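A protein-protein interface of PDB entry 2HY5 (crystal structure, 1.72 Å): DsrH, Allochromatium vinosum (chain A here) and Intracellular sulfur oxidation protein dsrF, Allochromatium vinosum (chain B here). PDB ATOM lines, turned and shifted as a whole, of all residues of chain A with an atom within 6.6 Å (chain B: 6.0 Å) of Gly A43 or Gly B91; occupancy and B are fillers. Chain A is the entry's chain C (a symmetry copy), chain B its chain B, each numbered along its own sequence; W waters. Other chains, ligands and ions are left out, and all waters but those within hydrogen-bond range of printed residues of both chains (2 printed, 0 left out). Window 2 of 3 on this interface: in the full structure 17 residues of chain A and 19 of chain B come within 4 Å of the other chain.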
ATOM      1  N   LEU A  41       0.853 -26.191  23.287  1.00  0.00           N
ATOM      2  CA  LEU A  41       1.800 -25.842  22.234  1.00  0.00           C
ATOM      3  C   LEU A  41       1.828 -26.792  21.038  1.00  0.00           C
ATOM      4  O   LEU A  41       1.866 -28.013  21.188  1.00  0.00           O
ATOM      5  CB  LEU A  41       3.197 -25.727  22.835  1.00  0.00           C
ATOM      6  CG  LEU A  41       3.288 -24.747  24.007  1.00  0.00           C
ATOM      7  CD1 LEU A  41       4.717 -24.713  24.521  1.00  0.00           C
ATOM      8  CD2 LEU A  41       2.840 -23.358  23.564  1.00  0.00           C
ATOM      9  N   ALA A  42       1.810 -26.219  19.841  1.00  0.00           N
ATOM     10  CA  ALA A  42       1.844 -27.020  18.628  1.00  0.00           C
ATOM     11  C   ALA A  42       3.205 -27.700  18.510  1.00  0.00           C
ATOM     12  O   ALA A  42       4.217 -27.158  18.954  1.00  0.00           O
ATOM     13  CB  ALA A  42       1.596 -26.136  17.413  1.00  0.00           C
ATOM     14  N   GLY A  43       3.216 -28.895  17.933  1.00  0.00           N
ATOM     15  CA  GLY A  43       4.462 -29.614  17.729  1.00  0.00           C
ATOM     16  C   GLY A  43       4.985 -30.544  18.810  1.00  0.00           C
ATOM     17  O   GLY A  43       6.004 -31.203  18.599  1.00  0.00           O
ATOM     18  N   THR A  44       4.315 -30.617  19.956  1.00  0.00           N
ATOM     19  CA  THR A  44       4.786 -31.499  21.026  1.00  0.00           C
ATOM     20  C   THR A  44       4.316 -32.931  20.811  1.00  0.00           C
ATOM     21  O   THR A  44       3.518 -33.209  19.913  1.00  0.00           O
ATOM     22  CB  THR A  44       4.287 -31.059  22.407  1.00  0.00           C
ATOM     23  OG1 THR A  44       2.940 -31.511  22.587  1.00  0.00           O
ATOM     24  CG2 THR A  44       4.344 -29.544  22.548  1.00  0.00           C
ATOM     25  N   ARG A  45       4.806 -33.835  21.652  1.00  0.00           N
ATOM     26  CA  ARG A  45       4.451 -35.245  21.560  1.00  0.00           C
ATOM     27  C   ARG A  45       2.995 -35.511  21.952  1.00  0.00           C
ATOM     28  O   ARG A  45       2.480 -36.606  21.724  1.00  0.00           O
ATOM     29  CB  ARG A  45       5.383 -36.074  22.448  1.00  0.00           C
ATOM     30  CG  ARG A  45       5.377 -37.560  22.136  1.00  0.00           C
ATOM     31  CD  ARG A  45       6.186 -38.350  23.153  1.00  0.00           C
ATOM     32  NE  ARG A  45       5.617 -38.245  24.494  1.00  0.00           N
ATOM     33  CZ  ARG A  45       6.123 -37.495  25.469  1.00  0.00           C
ATOM     34  NH1 ARG A  45       7.217 -36.779  25.258  1.00  0.00           N
ATOM     35  NH2 ARG A  45       5.531 -37.458  26.654  1.00  0.00           N
ATOM     36  N   VAL A  46       2.329 -34.520  22.542  1.00  0.00           N
ATOM     37  CA  VAL A  46       0.937 -34.705  22.941  1.00  0.00           C
ATOM     38  C   VAL A  46      -0.048 -33.926  22.080  1.00  0.00           C
ATOM     39  O   VAL A  46      -1.242 -33.916  22.366  1.00  0.00           O
ATOM     40  CB  VAL A  46       0.701 -34.318  24.426  1.00  0.00           C
ATOM     41  CG1 VAL A  46       1.621 -35.125  25.326  1.00  0.00           C
ATOM     42  CG2 VAL A  46       0.918 -32.827  24.626  1.00  0.00           C
ATOM     43  N   GLU A  47       0.443 -33.280  21.027  1.00  0.00           N
ATOM     44  CA  GLU A  47      -0.431 -32.506  20.146  1.00  0.00           C
ATOM     45  C   GLU A  47      -1.581 -33.353  19.599  1.00  0.00           C
ATOM     46  O   GLU A  47      -2.723 -32.901  19.545  1.00  0.00           O
ATOM     47  CB  GLU A  47       0.359 -31.917  18.972  1.00  0.00           C
ATOM     48  CG  GLU A  47      -0.486 -31.024  18.068  1.00  0.00           C
ATOM     49  CD  GLU A  47       0.221 -30.618  16.787  1.00  0.00           C
ATOM     50  OE1 GLU A  47       1.338 -30.073  16.863  1.00  0.00           O
ATOM     51  OE2 GLU A  47      -0.350 -30.839  15.698  1.00  0.00           O
ATOM     52  N   ARG A  75       1.818 -19.708  18.933  1.00  0.00           N
ATOM     53  CA  ARG A  75       2.469 -20.995  19.143  1.00  0.00           C
ATOM     54  C   ARG A  75       1.492 -22.058  19.622  1.00  0.00           C
ATOM     55  O   ARG A  75       1.843 -23.229  19.726  1.00  0.00           O
ATOM     56  CB  ARG A  75       3.593 -20.846  20.173  1.00  0.00           C
ATOM     57  CG  ARG A  75       4.680 -19.857  19.780  1.00  0.00           C
ATOM     58  CD  ARG A  75       5.449 -20.336  18.561  1.00  0.00           C
ATOM     59  NE  ARG A  75       6.353 -21.444  18.864  1.00  0.00           N
ATOM     60  CZ  ARG A  75       7.485 -21.322  19.553  1.00  0.00           C
ATOM     61  NH1 ARG A  75       7.864 -20.137  20.018  1.00  0.00           N
ATOM     62  NH2 ARG A  75       8.244 -22.386  19.775  1.00  0.00           N
ATOM     63  N   ILE A  77      -1.874 -24.581  19.659  1.00  0.00           N
ATOM     64  CA  ILE A  77      -2.574 -25.445  18.718  1.00  0.00           C
ATOM     65  C   ILE A  77      -3.860 -24.714  18.347  1.00  0.00           C
ATOM     66  O   ILE A  77      -4.628 -24.315  19.225  1.00  0.00           O
ATOM     67  CB  ILE A  77      -2.943 -26.792  19.371  1.00  0.00           C
ATOM     68  CG1 ILE A  77      -1.669 -27.546  19.763  1.00  0.00           C
ATOM     69  CG2 ILE A  77      -3.792 -27.626  18.412  1.00  0.00           C
ATOM     70  CD1 ILE A  77      -1.928 -28.757  20.645  1.00  0.00           C
ATOM     71  N   SER B  86      14.624 -34.442  24.542  1.00  0.00           N
ATOM     72  CA  SER B  86      13.673 -33.636  25.304  1.00  0.00           C
ATOM     73  C   SER B  86      13.170 -32.465  24.462  1.00  0.00           C
ATOM     74  O   SER B  86      11.986 -32.125  24.501  1.00  0.00           O
ATOM     75  CB  SER B  86      14.331 -33.115  26.578  1.00  0.00           C
ATOM     76  OG  SER B  86      14.697 -34.194  27.416  1.00  0.00           O
ATOM     77  N   LEU B  87      14.071 -31.847  23.706  1.00  0.00           N
ATOM     78  CA  LEU B  87      13.699 -30.731  22.847  1.00  0.00           C
ATOM     79  C   LEU B  87      12.701 -31.195  21.796  1.00  0.00           C
ATOM     80  O   LEU B  87      11.682 -30.548  21.573  1.00  0.00           O
ATOM     81  CB  LEU B  87      14.933 -30.151  22.147  1.00  0.00           C
ATOM     82  CG  LEU B  87      15.932 -29.351  22.980  1.00  0.00           C
ATOM     83  CD1 LEU B  87      17.076 -28.888  22.086  1.00  0.00           C
ATOM     84  CD2 LEU B  87      15.225 -28.151  23.604  1.00  0.00           C
ATOM     85  N   GLU B  88      13.002 -32.317  21.149  1.00  0.00           N
ATOM     86  CA  GLU B  88      12.132 -32.862  20.108  1.00  0.00           C
ATOM     87  C   GLU B  88      10.746 -33.214  20.634  1.00  0.00           C
ATOM     88  O   GLU B  88       9.731 -32.912  19.997  1.00  0.00           O
ATOM     89  CB  GLU B  88      12.765 -34.110  19.485  1.00  0.00           C
ATOM     90  CG  GLU B  88      11.896 -34.786  18.431  1.00  0.00           C
ATOM     91  CD  GLU B  88      12.486 -36.091  17.932  1.00  0.00           C
ATOM     92  OE1 GLU B  88      12.687 -37.013  18.755  1.00  0.00           O
ATOM     93  OE2 GLU B  88      12.743 -36.197  16.715  1.00  0.00           O
ATOM     94  N   ALA B  89      10.701 -33.862  21.794  1.00  0.00           N
ATOM     95  CA  ALA B  89       9.431 -34.255  22.385  1.00  0.00           C
ATOM     96  C   ALA B  89       8.555 -33.033  22.645  1.00  0.00           C
ATOM     97  O   ALA B  89       7.330 -33.134  22.724  1.00  0.00           O
ATOM     98  CB  ALA B  89       9.679 -35.012  23.685  1.00  0.00           C
ATOM     99  N   ARG B  90       9.188 -31.873  22.754  1.00  0.00           N
ATOM    100  CA  ARG B  90       8.464 -30.643  23.029  1.00  0.00           C
ATOM    101  C   ARG B  90       8.356 -29.732  21.804  1.00  0.00           C
ATOM    102  O   ARG B  90       7.940 -28.578  21.905  1.00  0.00           O
ATOM    103  CB  ARG B  90       9.137 -29.941  24.212  1.00  0.00           C
ATOM    104  CG  ARG B  90       9.063 -30.803  25.464  1.00  0.00           C
ATOM    105  CD  ARG B  90       9.935 -30.334  26.611  1.00  0.00           C
ATOM    106  NE  ARG B  90       9.700 -31.154  27.800  1.00  0.00           N
ATOM    107  CZ  ARG B  90      10.032 -32.440  27.904  1.00  0.00           C
ATOM    108  NH1 ARG B  90      10.626 -33.068  26.895  1.00  0.00           N
ATOM    109  NH2 ARG B  90       9.750 -33.110  29.012  1.00  0.00           N
ATOM    110  N   GLY B  91       8.714 -30.273  20.643  1.00  0.00           N
ATOM    111  CA  GLY B  91       8.648 -29.509  19.410  1.00  0.00           C
ATOM    112  C   GLY B  91       9.535 -28.281  19.420  1.00  0.00           C
ATOM    113  O   GLY B  91       9.228 -27.275  18.778  1.00  0.00           O
ATOM    114  N   LEU B  92      10.644 -28.360  20.146  1.00  0.00           N
ATOM    115  CA  LEU B  92      11.566 -27.240  20.228  1.00  0.00           C
ATOM    116  C   LEU B  92      12.861 -27.538  19.492  1.00  0.00           C
ATOM    117  O   LEU B  92      13.208 -28.695  19.265  1.00  0.00           O
ATOM    118  CB  LEU B  92      11.891 -26.923  21.691  1.00  0.00           C
ATOM    119  CG  LEU B  92      10.744 -26.565  22.635  1.00  0.00           C
ATOM    120  CD1 LEU B  92      11.305 -26.373  24.033  1.00  0.00           C
ATOM    121  CD2 LEU B  92      10.042 -25.300  22.159  1.00  0.00           C
ATOM    122  N   THR B  93      13.567 -26.479  19.114  1.00  0.00           N
ATOM    123  CA  THR B  93      14.848 -26.613  18.440  1.00  0.00           C
ATOM    124  C   THR B  93      15.779 -25.683  19.199  1.00  0.00           C
ATOM    125  O   THR B  93      15.321 -24.904  20.041  1.00  0.00           O
ATOM    126  CB  THR B  93      14.771 -26.174  16.964  1.00  0.00           C
ATOM    127  OG1 THR B  93      14.600 -24.753  16.889  1.00  0.00           O
ATOM    128  CG2 THR B  93      13.601 -26.853  16.274  1.00  0.00           C
ATOM    129  N   ASP B  96      14.925 -22.067  19.782  1.00  0.00           N
ATOM    130  CA  ASP B  96      13.948 -21.640  20.782  1.00  0.00           C
ATOM    131  C   ASP B  96      14.597 -21.324  22.122  1.00  0.00           C
ATOM    132  O   ASP B  96      13.940 -20.823  23.039  1.00  0.00           O
ATOM    133  CB  ASP B  96      12.898 -22.733  21.005  1.00  0.00           C
ATOM    134  CG  ASP B  96      11.981 -22.921  19.815  1.00  0.00           C
ATOM    135  OD1 ASP B  96      12.011 -24.014  19.212  1.00  0.00           O
ATOM    136  OD2 ASP B  96      11.231 -21.975  19.493  1.00  0.00           O
HETATM  137  O   HOH W   1       7.034 -33.779  18.908  1.00  0.00           O
HETATM  138  O   HOH W   2      10.807 -19.665  20.954  1.00  0.00           O
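The backbone NH (N) of Arg A45 lies within hydrogen-bond range of the backbone carbonyl oxygen (O) of Ala B89, at 2.8 Å. OD2 of Asp B96 lies within salt-bridge range of NH2 of Arg A75 (3.0 Å).
The backbone carbonyl oxygen of Ser B86 is in hydrogen-bond range of the guanidinium group of Arg B90, at 2.9 Å. N of Thr B93 lies within hydrogen-bond range of OD1 of Asp B96 (2.9 Å). O of Arg A75 is in hydrogen-bond range of N of Ala A42 (3.0 Å). The backbone NH (N) of Gly A43 is in hydrogen-bond range of the side-chain carboxylate (OE1) of Glu A47 (2.5 Å). The side-chain hydroxyl (OG1) of Thr A44 sits at hydrogen-bond distance from the backbone NH (N) of Val A46 (3.1 Å). OG1 of Thr A44 is in hydrogen-bond range of N of Glu A47, 3.4 Å away.
Gly A43 touches Gly B91. CA of Thr A44 touches O of Ala B89 (3.5 Å). CG2 of Thr A44 touches O of Arg B90 (3.8 Å).
Gly A43 touches just one residue of chain B: Gly B91. Gly B91 touches just one residue of chain A: Gly A43 (3.2 Å). Of the printed residues of chain B, Arg A45 touches Ala B89 (2.8 Å). Printed residues of chain B within 4 Å of Thr A44: Ala B89 (3.5 Å) and Arg B90 (3.8 Å). Printed residues of chain A within 4 Å of Ala B89: Thr A44 and Arg A45. Of the printed residues of chain A, Asp B96 touches Arg A75. The nearest residue of chain B that does not touch Gly A43 is Arg B90 (4.2 Å). The nearest residue of chain A that does not touch Gly B91 is Thr A44 (4.1 Å). The nearest printed residue of chain B that does not touch Thr A44 is Gly B91 (4.1 Å).
Of the 9 printed residues of chain B, 4 touch a printed residue of chain A. Printed residues of chain B that touch a printed residue of chain A: Ala B89, Arg B90, Gly B91 and Asp B96. Hydrophobic or aromatic side chains of chain B within 4 Å of the printed part of chain A: Ala B89. Among the printed residues, Asp or Glu carboxylates within 4 Å of a Lys or Arg side-chain nitrogen of the other chain: Arg A75 with Asp B96 (3.0 Å).
Water W2 bridges the side-chain carboxylate of Asp B96 (2.8 Å) and the guanidinium group of Arg A75 (3.1 Å). Water W1 bridges the backbone carbonyl oxygen (O) of Gly A43 (2.8 Å) and the backbone carbonyl oxygen (O) of Glu B88 (3.0 Å).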
